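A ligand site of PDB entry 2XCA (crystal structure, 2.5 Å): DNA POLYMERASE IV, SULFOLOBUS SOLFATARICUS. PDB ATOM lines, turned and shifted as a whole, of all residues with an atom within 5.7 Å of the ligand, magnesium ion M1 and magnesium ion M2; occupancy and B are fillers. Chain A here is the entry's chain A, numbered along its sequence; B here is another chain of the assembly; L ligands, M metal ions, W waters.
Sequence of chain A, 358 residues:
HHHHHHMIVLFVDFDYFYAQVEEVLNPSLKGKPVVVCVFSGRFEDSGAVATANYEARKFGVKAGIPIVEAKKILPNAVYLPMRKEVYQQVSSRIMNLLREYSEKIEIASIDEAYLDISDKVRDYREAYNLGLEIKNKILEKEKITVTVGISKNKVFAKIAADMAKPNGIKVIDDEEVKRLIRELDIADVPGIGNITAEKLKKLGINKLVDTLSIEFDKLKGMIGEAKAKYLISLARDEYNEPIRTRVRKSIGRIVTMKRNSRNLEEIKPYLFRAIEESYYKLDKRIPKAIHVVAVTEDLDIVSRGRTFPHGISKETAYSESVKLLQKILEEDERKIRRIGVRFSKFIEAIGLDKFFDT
NH1 of Arg 57 lies within salt-bridge range of O1 of the ligand.
The side-chain hydroxyl (OG1) of Thr 51 lies within hydrogen-bond range of an oxygen (O5) of the ligand, 2.7 Å away.
O2 of DC 4 of chain B sits at hydrogen-bond distance from a nitrogen (N4) of the ligand (2.8 Å).
The side-chain amino group (NZ) of Lys 165 is in salt-bridge range of an oxygen (O3) of the ligand (2.8 Å).
The backbone NH (N) of Tyr 16 sits at hydrogen-bond distance from an oxygen (O3) of the ligand (2.9 Å).
The side-chain hydroxyl (OH) of Tyr 54 sits at hydrogen-bond distance from an oxygen (O3) of the ligand.
A nitrogen (N3) of the ligand is in hydrogen-bond range of N2 of 8OG 5 of chain B (3.1 Å).
An oxygen (O6) of the ligand lies close to the backbone NH of Phe 17, 3.2 Å away.
The backbone NH of Tyr 18 sits at hydrogen-bond distance from an oxygen (O12) of the ligand (3.4 Å).
O of Phe 14 sits close to NZ of Lys 165 (3.1 Å).
N of Asp 111 lies within hydrogen-bond range of OG of Ser 109.
O of Asp 13 lies within hydrogen-bond range of NZ of Lys 165 (3.1 Å).
The backbone NH (N) of Glu 112 lies close to the side-chain hydroxyl (OG) of Ser 109 (3.3 Å).
The side-chain amino group (NZ) of Lys 158 is in salt-bridge range of the side-chain carboxylate (OE1) of Glu 112, at 3.1 Å.
The guanidinium group (NH2) of Arg 57 is in hydrogen-bond range of the side-chain hydroxyl (OG1) of Thr 51, 3.3 Å away.
The guanidinium group (NE) of Arg 57 lies within hydrogen-bond range of the backbone carbonyl oxygen (O) of Ala 52 (2.9 Å).
NZ of Lys 165 is in salt-bridge range of OD1 of Asp 15, at 2.9 Å.
Asp 15 touches the ligand.
Val 38 touches the ligand.
Ala 50 touches the ligand.
Ala 63 touches the ligand.
Ile 110 touches the ligand (CG2 to O11, 3.99 Å).
17 residues have an atom within 4 Å of the ligand: Asp 13, Phe 14, Asp 15, Tyr 16, Phe 17, Tyr 18, Val 38, Ala 50, Thr 51, Tyr 54, Arg 57, Ala 63, Ile 110, Asp 111, Lys 165, DC 4 of chain B and 8OG 5 of chain B.
Along chain A the residues within 4 Å of the ligand span positions 13 to 165.
The nearest printed residue that does not touch the ligand is Met 82 (4.2 Å).
Ser 109 touches magnesium ion M1 (OG to MG, 3.7 Å).
Residues that only touch magnesium ion M2: Lys 165 (3.2 Å).
The nearest printed residue that does not touch magnesium ion M2 is Asp 15 (4.1 Å).
The side-chain carboxylate (OD1) of Asp 111 binds magnesium ion M1.
OD1 of Asp 13 binds magnesium ion M1, at 2.1 Å.
Water W5 is bound to magnesium ion M1 (2.2 Å).
OE2 of Glu 112 binds magnesium ion M1 (2.3 Å).
Water W3 is bound to magnesium ion M1, 2.3 Å away.
Magnesium ion M1 is bound by an oxygen (O8) of the ligand (2.4 Å).
Magnesium ion M1 has six donor atoms within binding distance.
Magnesium ion M2 is bound by O of Phe 14 (2.0 Å), O6 of the ligand (2.1 Å), O2 of the ligand (2.2 Å), O8 of the ligand (2.2 Å), OD2 of Asp 13 (2.2 Å) and OD2 of Asp 111 (2.3 Å).
Water W5 lies within hydrogen-bond range of an oxygen (O9) of the ligand (3.0 Å) and the side-chain amino group of Lys 158 (3.0 Å).
Water W3 bridges O10 of the ligand (3.0 Å) and OG of Ser 109 (3.4 Å).
Water W6 lies within hydrogen-bond range of the side-chain hydroxyl (OH) of Tyr 18 and a nitrogen (N5) of the ligand.
Water W2 lies within hydrogen-bond range of N1 of 8OG 5 of chain B (3.3 Å) and O13 of the ligand (3.5 Å).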
ATOM      1  N   PHE A  11      21.905  15.409   1.514  1.00  0.00           N
ATOM      2  CA  PHE A  11      20.877  15.665   0.509  1.00  0.00           C
ATOM      3  C   PHE A  11      20.133  14.373   0.186  1.00  0.00           C
ATOM      4  O   PHE A  11      20.733  13.304   0.050  1.00  0.00           O
ATOM      5  CB  PHE A  11      21.545  16.228  -0.758  1.00  0.00           C
ATOM      6  CG  PHE A  11      20.676  16.183  -1.989  1.00  0.00           C
ATOM      7  CD1 PHE A  11      19.753  17.201  -2.260  1.00  0.00           C
ATOM      8  CD2 PHE A  11      20.825  15.146  -2.925  1.00  0.00           C
ATOM      9  CE1 PHE A  11      18.991  17.182  -3.451  1.00  0.00           C
ATOM     10  CE2 PHE A  11      20.065  15.130  -4.092  1.00  0.00           C
ATOM     11  CZ  PHE A  11      19.148  16.154  -4.368  1.00  0.00           C
ATOM     12  N   ASP A  13      17.063  12.589  -2.365  1.00  0.00           N
ATOM     13  CA  ASP A  13      16.317  12.676  -3.611  1.00  0.00           C
ATOM     14  C   ASP A  13      15.555  11.355  -3.839  1.00  0.00           C
ATOM     15  O   ASP A  13      16.171  10.298  -3.871  1.00  0.00           O
ATOM     16  CB  ASP A  13      17.275  12.935  -4.755  1.00  0.00           C
ATOM     17  CG  ASP A  13      16.551  13.347  -6.023  1.00  0.00           C
ATOM     18  OD1 ASP A  13      16.239  14.538  -6.149  1.00  0.00           O
ATOM     19  OD2 ASP A  13      16.297  12.470  -6.865  1.00  0.00           O
ATOM     20  N   PHE A  14      14.233  11.426  -4.008  1.00  0.00           N
ATOM     21  CA  PHE A  14      13.430  10.215  -4.202  1.00  0.00           C
ATOM     22  C   PHE A  14      13.701   9.554  -5.564  1.00  0.00           C
ATOM     23  O   PHE A  14      13.799  10.220  -6.566  1.00  0.00           O
ATOM     24  CB  PHE A  14      11.934  10.526  -4.078  1.00  0.00           C
ATOM     25  CG  PHE A  14      11.604  11.434  -2.932  1.00  0.00           C
ATOM     26  CD1 PHE A  14      12.500  11.611  -1.884  1.00  0.00           C
ATOM     27  CD2 PHE A  14      10.413  12.141  -2.929  1.00  0.00           C
ATOM     28  CE1 PHE A  14      12.205  12.495  -0.833  1.00  0.00           C
ATOM     29  CE2 PHE A  14      10.103  13.017  -1.905  1.00  0.00           C
ATOM     30  CZ  PHE A  14      11.003  13.210  -0.835  1.00  0.00           C
ATOM     31  N   ASP A  15      13.797   8.233  -5.620  1.00  0.00           N
ATOM     32  CA  ASP A  15      14.080   7.596  -6.887  1.00  0.00           C
ATOM     33  C   ASP A  15      12.899   7.589  -7.863  1.00  0.00           C
ATOM     34  O   ASP A  15      11.765   7.356  -7.451  1.00  0.00           O
ATOM     35  CB  ASP A  15      14.598   6.184  -6.646  1.00  0.00           C
ATOM     36  CG  ASP A  15      15.922   6.185  -5.899  1.00  0.00           C
ATOM     37  OD1 ASP A  15      16.678   7.177  -6.006  1.00  0.00           O
ATOM     38  OD2 ASP A  15      16.229   5.195  -5.217  1.00  0.00           O
ATOM     39  N   TYR A  16      13.172   7.852  -9.142  1.00  0.00           N
ATOM     40  CA  TYR A  16      12.125   7.889 -10.195  1.00  0.00           C
ATOM     41  C   TYR A  16      10.767   8.122  -9.569  1.00  0.00           C
ATOM     42  O   TYR A  16       9.793   7.428  -9.844  1.00  0.00           O
ATOM     43  CB  TYR A  16      12.160   6.572 -11.017  1.00  0.00           C
ATOM     44  CG  TYR A  16      11.924   5.286 -10.233  1.00  0.00           C
ATOM     45  CD1 TYR A  16      10.655   4.683 -10.216  1.00  0.00           C
ATOM     46  CD2 TYR A  16      12.957   4.676  -9.520  1.00  0.00           C
ATOM     47  CE1 TYR A  16      10.428   3.514  -9.521  1.00  0.00           C
ATOM     48  CE2 TYR A  16      12.722   3.488  -8.818  1.00  0.00           C
ATOM     49  CZ  TYR A  16      11.456   2.918  -8.817  1.00  0.00           C
ATOM     50  OH  TYR A  16      11.200   1.765  -8.083  1.00  0.00           O
ATOM     51  N   PHE A  17      10.721   9.166  -8.748  1.00  0.00           N
ATOM     52  CA  PHE A  17       9.566   9.566  -7.955  1.00  0.00           C
ATOM     53  C   PHE A  17       8.130   9.397  -8.432  1.00  0.00           C
ATOM     54  O   PHE A  17       7.389   8.642  -7.800  1.00  0.00           O
ATOM     55  CB  PHE A  17       9.767  10.993  -7.429  1.00  0.00           C
ATOM     56  CG  PHE A  17       8.805  11.369  -6.327  1.00  0.00           C
ATOM     57  CD1 PHE A  17       8.588  10.520  -5.247  1.00  0.00           C
ATOM     58  CD2 PHE A  17       8.100  12.556  -6.392  1.00  0.00           C
ATOM     59  CE1 PHE A  17       7.680  10.848  -4.245  1.00  0.00           C
ATOM     60  CE2 PHE A  17       7.183  12.906  -5.395  1.00  0.00           C
ATOM     61  CZ  PHE A  17       6.975  12.041  -4.322  1.00  0.00           C
ATOM     62  N   TYR A  18       7.714  10.074  -9.493  1.00  0.00           N
ATOM     63  CA  TYR A  18       6.316   9.948  -9.937  1.00  0.00           C
ATOM     64  C   TYR A  18       5.966   8.532 -10.308  1.00  0.00           C
ATOM     65  O   TYR A  18       4.866   8.052 -10.042  1.00  0.00           O
ATOM     66  CB  TYR A  18       6.053  10.836 -11.158  1.00  0.00           C
ATOM     67  CG  TYR A  18       5.976  12.313 -10.882  1.00  0.00           C
ATOM     68  CD1 TYR A  18       6.437  12.839  -9.687  1.00  0.00           C
ATOM     69  CD2 TYR A  18       5.493  13.191 -11.847  1.00  0.00           C
ATOM     70  CE1 TYR A  18       6.402  14.219  -9.446  1.00  0.00           C
ATOM     71  CE2 TYR A  18       5.457  14.546 -11.632  1.00  0.00           C
ATOM     72  CZ  TYR A  18       5.912  15.067 -10.432  1.00  0.00           C
ATOM     73  OH  TYR A  18       5.881  16.408 -10.208  1.00  0.00           O
ATOM     74  N   ALA A  19       6.899   7.837 -10.946  1.00  0.00           N
ATOM     75  CA  ALA A  19       6.675   6.470 -11.360  1.00  0.00           C
ATOM     76  C   ALA A  19       6.607   5.579 -10.118  1.00  0.00           C
ATOM     77  O   ALA A  19       5.676   4.767  -9.968  1.00  0.00           O
ATOM     78  CB  ALA A  19       7.765   6.026 -12.294  1.00  0.00           C
ATOM     79  N   VAL A  38       2.461  13.359 -19.519  1.00  0.00           N
ATOM     80  CA  VAL A  38       1.706  14.581 -19.474  1.00  0.00           C
ATOM     81  C   VAL A  38       1.093  14.710 -20.875  1.00  0.00           C
ATOM     82  O   VAL A  38       1.756  15.193 -21.807  1.00  0.00           O
ATOM     83  CB  VAL A  38       2.606  15.793 -19.166  1.00  0.00           C
ATOM     84  CG1 VAL A  38       1.804  17.084 -19.307  1.00  0.00           C
ATOM     85  CG2 VAL A  38       3.181  15.671 -17.800  1.00  0.00           C
ATOM     86  N   VAL A  49       7.028  12.998 -21.548  1.00  0.00           N
ATOM     87  CA  VAL A  49       7.160  12.108 -20.425  1.00  0.00           C
ATOM     88  C   VAL A  49       7.618  12.870 -19.191  1.00  0.00           C
ATOM     89  O   VAL A  49       8.649  13.539 -19.228  1.00  0.00           O
ATOM     90  CB  VAL A  49       8.196  11.003 -20.727  1.00  0.00           C
ATOM     91  CG1 VAL A  49       8.500  10.231 -19.449  1.00  0.00           C
ATOM     92  CG2 VAL A  49       7.673  10.072 -21.824  1.00  0.00           C
ATOM     93  N   ALA A  50       6.858  12.787 -18.100  1.00  0.00           N
ATOM     94  CA  ALA A  50       7.254  13.473 -16.851  1.00  0.00           C
ATOM     95  C   ALA A  50       8.453  12.753 -16.266  1.00  0.00           C
ATOM     96  O   ALA A  50       9.426  13.394 -15.844  1.00  0.00           O
ATOM     97  CB  ALA A  50       6.123  13.478 -15.851  1.00  0.00           C
ATOM     98  N   THR A  51       8.379  11.428 -16.242  1.00  0.00           N
ATOM     99  CA  THR A  51       9.448  10.537 -15.782  1.00  0.00           C
ATOM    100  C   THR A  51       9.095   9.065 -16.031  1.00  0.00           C
ATOM    101  O   THR A  51       7.975   8.734 -16.369  1.00  0.00           O
ATOM    102  CB  THR A  51       9.758  10.677 -14.281  1.00  0.00           C
ATOM    103  OG1 THR A  51      11.029  10.067 -13.997  1.00  0.00           O
ATOM    104  CG2 THR A  51       8.671   9.976 -13.417  1.00  0.00           C
ATOM    105  N   ALA A  52      10.073   8.181 -15.834  1.00  0.00           N
ATOM    106  CA  ALA A  52       9.871   6.753 -16.029  1.00  0.00           C
ATOM    107  C   ALA A  52      10.732   6.000 -15.034  1.00  0.00           C
ATOM    108  O   ALA A  52      11.792   6.501 -14.659  1.00  0.00           O
ATOM    109  CB  ALA A  52      10.276   6.349 -17.430  1.00  0.00           C
ATOM    110  N   TYR A  54      13.318   3.052 -13.695  1.00  0.00           N
ATOM    111  CA  TYR A  54      14.602   2.659 -14.296  1.00  0.00           C
ATOM    112  C   TYR A  54      14.527   1.572 -15.355  1.00  0.00           C
ATOM    113  O   TYR A  54      15.368   1.526 -16.251  1.00  0.00           O
ATOM    114  CB  TYR A  54      15.610   2.288 -13.194  1.00  0.00           C
ATOM    115  CG  TYR A  54      16.150   3.520 -12.483  1.00  0.00           C
ATOM    116  CD1 TYR A  54      15.332   4.300 -11.681  1.00  0.00           C
ATOM    117  CD2 TYR A  54      17.467   3.909 -12.671  1.00  0.00           C
ATOM    118  CE1 TYR A  54      15.816   5.448 -11.067  1.00  0.00           C
ATOM    119  CE2 TYR A  54      17.974   5.060 -12.064  1.00  0.00           C
ATOM    120  CZ  TYR A  54      17.137   5.828 -11.258  1.00  0.00           C
ATOM    121  OH  TYR A  54      17.620   6.951 -10.616  1.00  0.00           O
ATOM    122  N   ARG A  57      14.078   3.491 -18.353  1.00  0.00           N
ATOM    123  CA  ARG A  57      15.185   4.390 -18.708  1.00  0.00           C
ATOM    124  C   ARG A  57      16.326   3.668 -19.394  1.00  0.00           C
ATOM    125  O   ARG A  57      17.177   4.301 -20.027  1.00  0.00           O
ATOM    126  CB  ARG A  57      15.753   5.102 -17.476  1.00  0.00           C
ATOM    127  CG  ARG A  57      14.826   6.119 -16.846  1.00  0.00           C
ATOM    128  CD  ARG A  57      15.511   6.852 -15.714  1.00  0.00           C
ATOM    129  NE  ARG A  57      14.524   7.476 -14.844  1.00  0.00           N
ATOM    130  CZ  ARG A  57      14.820   8.225 -13.773  1.00  0.00           C
ATOM    131  NH1 ARG A  57      16.097   8.444 -13.463  1.00  0.00           N
ATOM    132  NH2 ARG A  57      13.841   8.739 -13.028  1.00  0.00           N
ATOM    133  N   ALA A  63      12.299  11.561 -18.867  1.00  0.00           N
ATOM    134  CA  ALA A  63      11.669  12.882 -18.760  1.00  0.00           C
ATOM    135  C   ALA A  63      12.125  13.799 -19.901  1.00  0.00           C
ATOM    136  O   ALA A  63      13.304  13.880 -20.218  1.00  0.00           O
ATOM    137  CB  ALA A  63      12.025  13.515 -17.410  1.00  0.00           C
ATOM    138  N   GLY A  64      11.167  14.468 -20.521  1.00  0.00           N
ATOM    139  CA  GLY A  64      11.488  15.382 -21.599  1.00  0.00           C
ATOM    140  C   GLY A  64      11.130  14.930 -23.002  1.00  0.00           C
ATOM    141  O   GLY A  64      10.647  15.743 -23.795  1.00  0.00           O
ATOM    142  N   MET A  82       0.086  11.642 -15.596  1.00  0.00           N
ATOM    143  CA  MET A  82       0.649  12.257 -14.397  1.00  0.00           C
ATOM    144  C   MET A  82      -0.430  12.748 -13.420  1.00  0.00           C
ATOM    145  O   MET A  82      -1.323  13.512 -13.793  1.00  0.00           O
ATOM    146  CB  MET A  82       1.549  13.438 -14.787  1.00  0.00           C
ATOM    147  CG  MET A  82       2.145  14.170 -13.593  1.00  0.00           C
ATOM    148  SD  MET A  82       2.996  15.639 -14.089  1.00  0.00           S
ATOM    149  CE  MET A  82       1.608  16.782 -14.318  1.00  0.00           C
ATOM    150  N   SER A 109      12.878  20.898  -4.413  1.00  0.00           N
ATOM    151  CA  SER A 109      12.007  20.475  -5.506  1.00  0.00           C
ATOM    152  C   SER A 109      10.940  19.587  -4.908  1.00  0.00           C
ATOM    153  O   SER A 109      10.876  19.425  -3.690  1.00  0.00           O
ATOM    154  CB  SER A 109      12.794  19.662  -6.545  1.00  0.00           C
ATOM    155  OG  SER A 109      12.882  18.287  -6.186  1.00  0.00           O
ATOM    156  N   ILE A 110      10.092  19.019  -5.757  1.00  0.00           N
ATOM    157  CA  ILE A 110       9.036  18.145  -5.260  1.00  0.00           C
ATOM    158  C   ILE A 110       9.591  16.845  -4.710  1.00  0.00           C
ATOM    159  O   ILE A 110       8.860  16.073  -4.085  1.00  0.00           O
ATOM    160  CB  ILE A 110       8.039  17.825  -6.352  1.00  0.00           C
ATOM    161  CG1 ILE A 110       6.807  17.162  -5.746  1.00  0.00           C
ATOM    162  CG2 ILE A 110       8.690  16.911  -7.378  1.00  0.00           C
ATOM    163  CD1 ILE A 110       5.567  17.217  -6.632  1.00  0.00           C
ATOM    164  N   ASP A 111      10.881  16.568  -4.907  1.00  0.00           N
ATOM    165  CA  ASP A 111      11.397  15.292  -4.375  1.00  0.00           C
ATOM    166  C   ASP A 111      12.802  15.330  -3.831  1.00  0.00           C
ATOM    167  O   ASP A 111      13.469  14.289  -3.787  1.00  0.00           O
ATOM    168  CB  ASP A 111      11.303  14.199  -5.445  1.00  0.00           C
ATOM    169  CG  ASP A 111      12.449  14.289  -6.420  1.00  0.00           C
ATOM    170  OD1 ASP A 111      12.790  15.422  -6.817  1.00  0.00           O
ATOM    171  OD2 ASP A 111      12.983  13.228  -6.789  1.00  0.00           O
ATOM    172  N   GLU A 112      13.268  16.506  -3.412  1.00  0.00           N
ATOM    173  CA  GLU A 112      14.611  16.589  -2.854  1.00  0.00           C
ATOM    174  C   GLU A 112      14.763  17.680  -1.794  1.00  0.00           C
ATOM    175  O   GLU A 112      14.103  18.721  -1.830  1.00  0.00           O
ATOM    176  CB  GLU A 112      15.660  16.769  -3.957  1.00  0.00           C
ATOM    177  CG  GLU A 112      15.489  18.018  -4.785  1.00  0.00           C
ATOM    178  CD  GLU A 112      16.154  17.899  -6.162  1.00  0.00           C
ATOM    179  OE1 GLU A 112      17.365  18.141  -6.310  1.00  0.00           O
ATOM    180  OE2 GLU A 112      15.440  17.539  -7.101  1.00  0.00           O
ATOM    181  N   LYS A 158      24.620  17.014  -3.559  1.00  0.00           N
ATOM    182  CA  LYS A 158      23.801  16.711  -4.725  1.00  0.00           C
ATOM    183  C   LYS A 158      24.572  15.777  -5.670  1.00  0.00           C
ATOM    184  O   LYS A 158      24.051  14.780  -6.149  1.00  0.00           O
ATOM    185  CB  LYS A 158      23.437  18.015  -5.441  1.00  0.00           C
ATOM    186  CG  LYS A 158      22.753  17.865  -6.790  1.00  0.00           C
ATOM    187  CD  LYS A 158      21.393  17.265  -6.669  1.00  0.00           C
ATOM    188  CE  LYS A 158      20.729  17.097  -8.035  1.00  0.00           C
ATOM    189  NZ  LYS A 158      19.387  16.434  -7.942  1.00  0.00           N
ATOM    190  N   LYS A 165      22.807   7.109  -7.469  1.00  0.00           N
ATOM    191  CA  LYS A 165      21.466   6.742  -7.934  1.00  0.00           C
ATOM    192  C   LYS A 165      21.504   5.364  -8.613  1.00  0.00           C
ATOM    193  O   LYS A 165      22.434   5.086  -9.372  1.00  0.00           O
ATOM    194  CB  LYS A 165      20.952   7.786  -8.927  1.00  0.00           C
ATOM    195  CG  LYS A 165      20.363   9.056  -8.327  1.00  0.00           C
ATOM    196  CD  LYS A 165      18.917   8.845  -7.898  1.00  0.00           C
ATOM    197  CE  LYS A 165      18.313  10.100  -7.258  1.00  0.00           C
ATOM    198  NZ  LYS A 165      16.879   9.911  -6.865  1.00  0.00           N
ATOM    199  N   PRO A 166      20.510   4.495  -8.356  1.00  0.00           N
ATOM    200  CA  PRO A 166      19.343   4.683  -7.484  1.00  0.00           C
ATOM    201  C   PRO A 166      19.499   3.929  -6.172  1.00  0.00           C
ATOM    202  O   PRO A 166      20.442   3.147  -6.001  1.00  0.00           O
ATOM    203  CB  PRO A 166      18.211   4.133  -8.325  1.00  0.00           C
ATOM    204  CG  PRO A 166      18.856   2.940  -8.948  1.00  0.00           C
ATOM    205  CD  PRO A 166      20.240   3.430  -9.340  1.00  0.00           C
ATOM    206  P    DC B   4       5.203  20.551 -25.357  1.00  0.00           P
ATOM    207  OP1  DC B   4       4.241  20.873 -26.458  1.00  0.00           O
ATOM    208  OP2  DC B   4       6.370  21.418 -25.104  1.00  0.00           O
ATOM    209  O5'  DC B   4       4.416  20.294 -24.016  1.00  0.00           O
ATOM    210  C5'  DC B   4       3.513  19.189 -23.993  1.00  0.00           C
ATOM    211  C4'  DC B   4       3.093  18.866 -22.559  1.00  0.00           C
ATOM    212  O4'  DC B   4       4.200  18.332 -21.792  1.00  0.00           O
ATOM    213  C3'  DC B   4       2.719  20.172 -21.841  1.00  0.00           C
ATOM    214  O3'  DC B   4       1.629  19.901 -20.992  1.00  0.00           O
ATOM    215  C2'  DC B   4       3.976  20.538 -21.066  1.00  0.00           C
ATOM    216  C1'  DC B   4       4.524  19.187 -20.707  1.00  0.00           C
ATOM    217  N1   DC B   4       5.976  19.121 -20.532  1.00  0.00           N
ATOM    218  C2   DC B   4       6.491  18.672 -19.320  1.00  0.00           C
ATOM    219  O2   DC B   4       5.704  18.403 -18.416  1.00  0.00           O
ATOM    220  N3   DC B   4       7.824  18.527 -19.161  1.00  0.00           N
ATOM    221  C4   DC B   4       8.649  18.811 -20.191  1.00  0.00           C
ATOM    222  N4   DC B   4       9.950  18.593 -20.016  1.00  0.00           N
ATOM    223  C5   DC B   4       8.159  19.318 -21.423  1.00  0.00           C
ATOM    224  C6   DC B   4       6.834  19.467 -21.551  1.00  0.00           C
ATOM    225  P   8OG B   5       0.646  21.095 -20.553  1.00  0.00           P
ATOM    226  OP1 8OG B   5      -0.671  20.539 -20.153  1.00  0.00           O
ATOM    227  OP2 8OG B   5       0.694  22.135 -21.608  1.00  0.00           O
ATOM    228  O5' 8OG B   5       1.335  21.664 -19.239  1.00  0.00           O
ATOM    229  C5' 8OG B   5       1.491  20.777 -18.123  1.00  0.00           C
ATOM    230  C4' 8OG B   5       2.686  21.203 -17.283  1.00  0.00           C
ATOM    231  O4' 8OG B   5       3.905  21.224 -18.043  1.00  0.00           O
ATOM    232  C3' 8OG B   5       2.571  22.631 -16.749  1.00  0.00           C
ATOM    233  O3' 8OG B   5       1.933  22.579 -15.447  1.00  0.00           O
ATOM    234  C2' 8OG B   5       4.024  23.101 -16.659  1.00  0.00           C
ATOM    235  C1' 8OG B   5       4.816  21.876 -17.144  1.00  0.00           C
ATOM    236  N9  8OG B   5       6.092  22.163 -17.837  1.00  0.00           N
ATOM    237  C8  8OG B   5       6.247  22.794 -18.993  1.00  0.00           C
ATOM    238  N7  8OG B   5       7.502  22.706 -19.439  1.00  0.00           N
ATOM    239  C5  8OG B   5       8.156  22.022 -18.517  1.00  0.00           C
ATOM    240  C6  8OG B   5       9.489  21.650 -18.448  1.00  0.00           C
ATOM    241  O6  8OG B   5      10.300  21.880 -19.347  1.00  0.00           O
ATOM    242  N1  8OG B   5       9.883  20.941 -17.315  1.00  0.00           N
ATOM    243  C2  8OG B   5       8.956  20.617 -16.316  1.00  0.00           C
ATOM    244  N2  8OG B   5       9.346  19.958 -15.246  1.00  0.00           N
ATOM    245  N3  8OG B   5       7.662  20.995 -16.406  1.00  0.00           N
ATOM    246  C4  8OG B   5       7.288  21.673 -17.476  1.00  0.00           C
ATOM    247  O8  8OG B   5       5.312  23.369 -19.539  1.00  0.00           O
HETATM  248  P1  LIG L   1      15.736  10.048 -10.199  1.00  0.00           P
HETATM  249  O1  LIG L   1      16.935  10.074 -11.271  1.00  0.00           O
HETATM  250  O2  LIG L   1      15.833  11.450  -9.412  1.00  0.00           O
HETATM  251  O3  LIG L   1      15.837   8.875  -9.297  1.00  0.00           O
HETATM  252  O4  LIG L   1      14.373  10.082 -11.045  1.00  0.00           O
HETATM  253  P2  LIG L   1      13.237  11.197 -10.829  1.00  0.00           P
HETATM  254  O5  LIG L   1      12.088  10.807 -11.670  1.00  0.00           O
HETATM  255  O6  LIG L   1      13.009  11.381  -9.381  1.00  0.00           O
HETATM  256  O7  LIG L   1      13.941  12.503 -11.461  1.00  0.00           O
HETATM  257  P3  LIG L   1      14.356  13.799 -10.605  1.00  0.00           P
HETATM  258  O8  LIG L   1      14.400  13.555  -9.017  1.00  0.00           O
HETATM  259  O9  LIG L   1      15.140  14.888 -11.225  1.00  0.00           O
HETATM  260  O10 LIG L   1      12.896  14.464 -10.660  1.00  0.00           O
HETATM  261  C1  LIG L   1      11.897  14.138  -9.691  1.00  0.00           C
HETATM  262  C2  LIG L   1      10.489  14.281 -10.288  1.00  0.00           C
HETATM  263  O11 LIG L   1      10.218  15.588 -10.820  1.00  0.00           O
HETATM  264  C3  LIG L   1      10.250  13.345 -11.472  1.00  0.00           C
HETATM  265  O12 LIG L   1       9.983  12.032 -10.991  1.00  0.00           O
HETATM  266  C4  LIG L   1       8.943  13.961 -11.976  1.00  0.00           C
HETATM  267  C5  LIG L   1       9.312  15.456 -11.925  1.00  0.00           C
HETATM  268  N1  LIG L   1      10.012  15.853 -13.165  1.00  0.00           N
HETATM  269  C6  LIG L   1      11.328  15.856 -13.388  1.00  0.00           C
HETATM  270  N2  LIG L   1      11.583  16.292 -14.616  1.00  0.00           N
HETATM  271  C7  LIG L   1      10.419  16.600 -15.187  1.00  0.00           C
HETATM  272  C8  LIG L   1      10.068  17.071 -16.446  1.00  0.00           C
HETATM  273  O13 LIG L   1      10.927  17.336 -17.308  1.00  0.00           O
HETATM  274  N3  LIG L   1       8.705  17.261 -16.740  1.00  0.00           N
HETATM  275  C9  LIG L   1       7.744  16.958 -15.776  1.00  0.00           C
HETATM  276  N4  LIG L   1       6.455  17.088 -16.067  1.00  0.00           N
HETATM  277  N5  LIG L   1       8.122  16.499 -14.566  1.00  0.00           N
HETATM  278  C10 LIG L   1       9.414  16.305 -14.265  1.00  0.00           C
HETATM  279 MG    MG M   1      14.776  15.405  -7.458  1.00  0.00          MG
HETATM  280 MG    MG M   2      14.422  11.692  -7.802  1.00  0.00          MG
HETATM  281  O   HOH W   1      13.831  17.313 -18.489  1.00  0.00           O
HETATM  282  O   HOH W   2      12.985  20.087 -17.920  1.00  0.00           O
HETATM  283  O   HOH W   3      13.873  16.761  -9.070  1.00  0.00           O
HETATM  284  O   HOH W   4      11.230  18.113  -9.671  1.00  0.00           O
HETATM  285  O   HOH W   5      16.646  15.435  -8.699  1.00  0.00           O
HETATM  286  O   HOH W   6       6.003  17.652 -12.647  1.00  0.00           O
HETATM  287  O   HOH W   7      17.950  12.684  -9.162  1.00  0.00           O
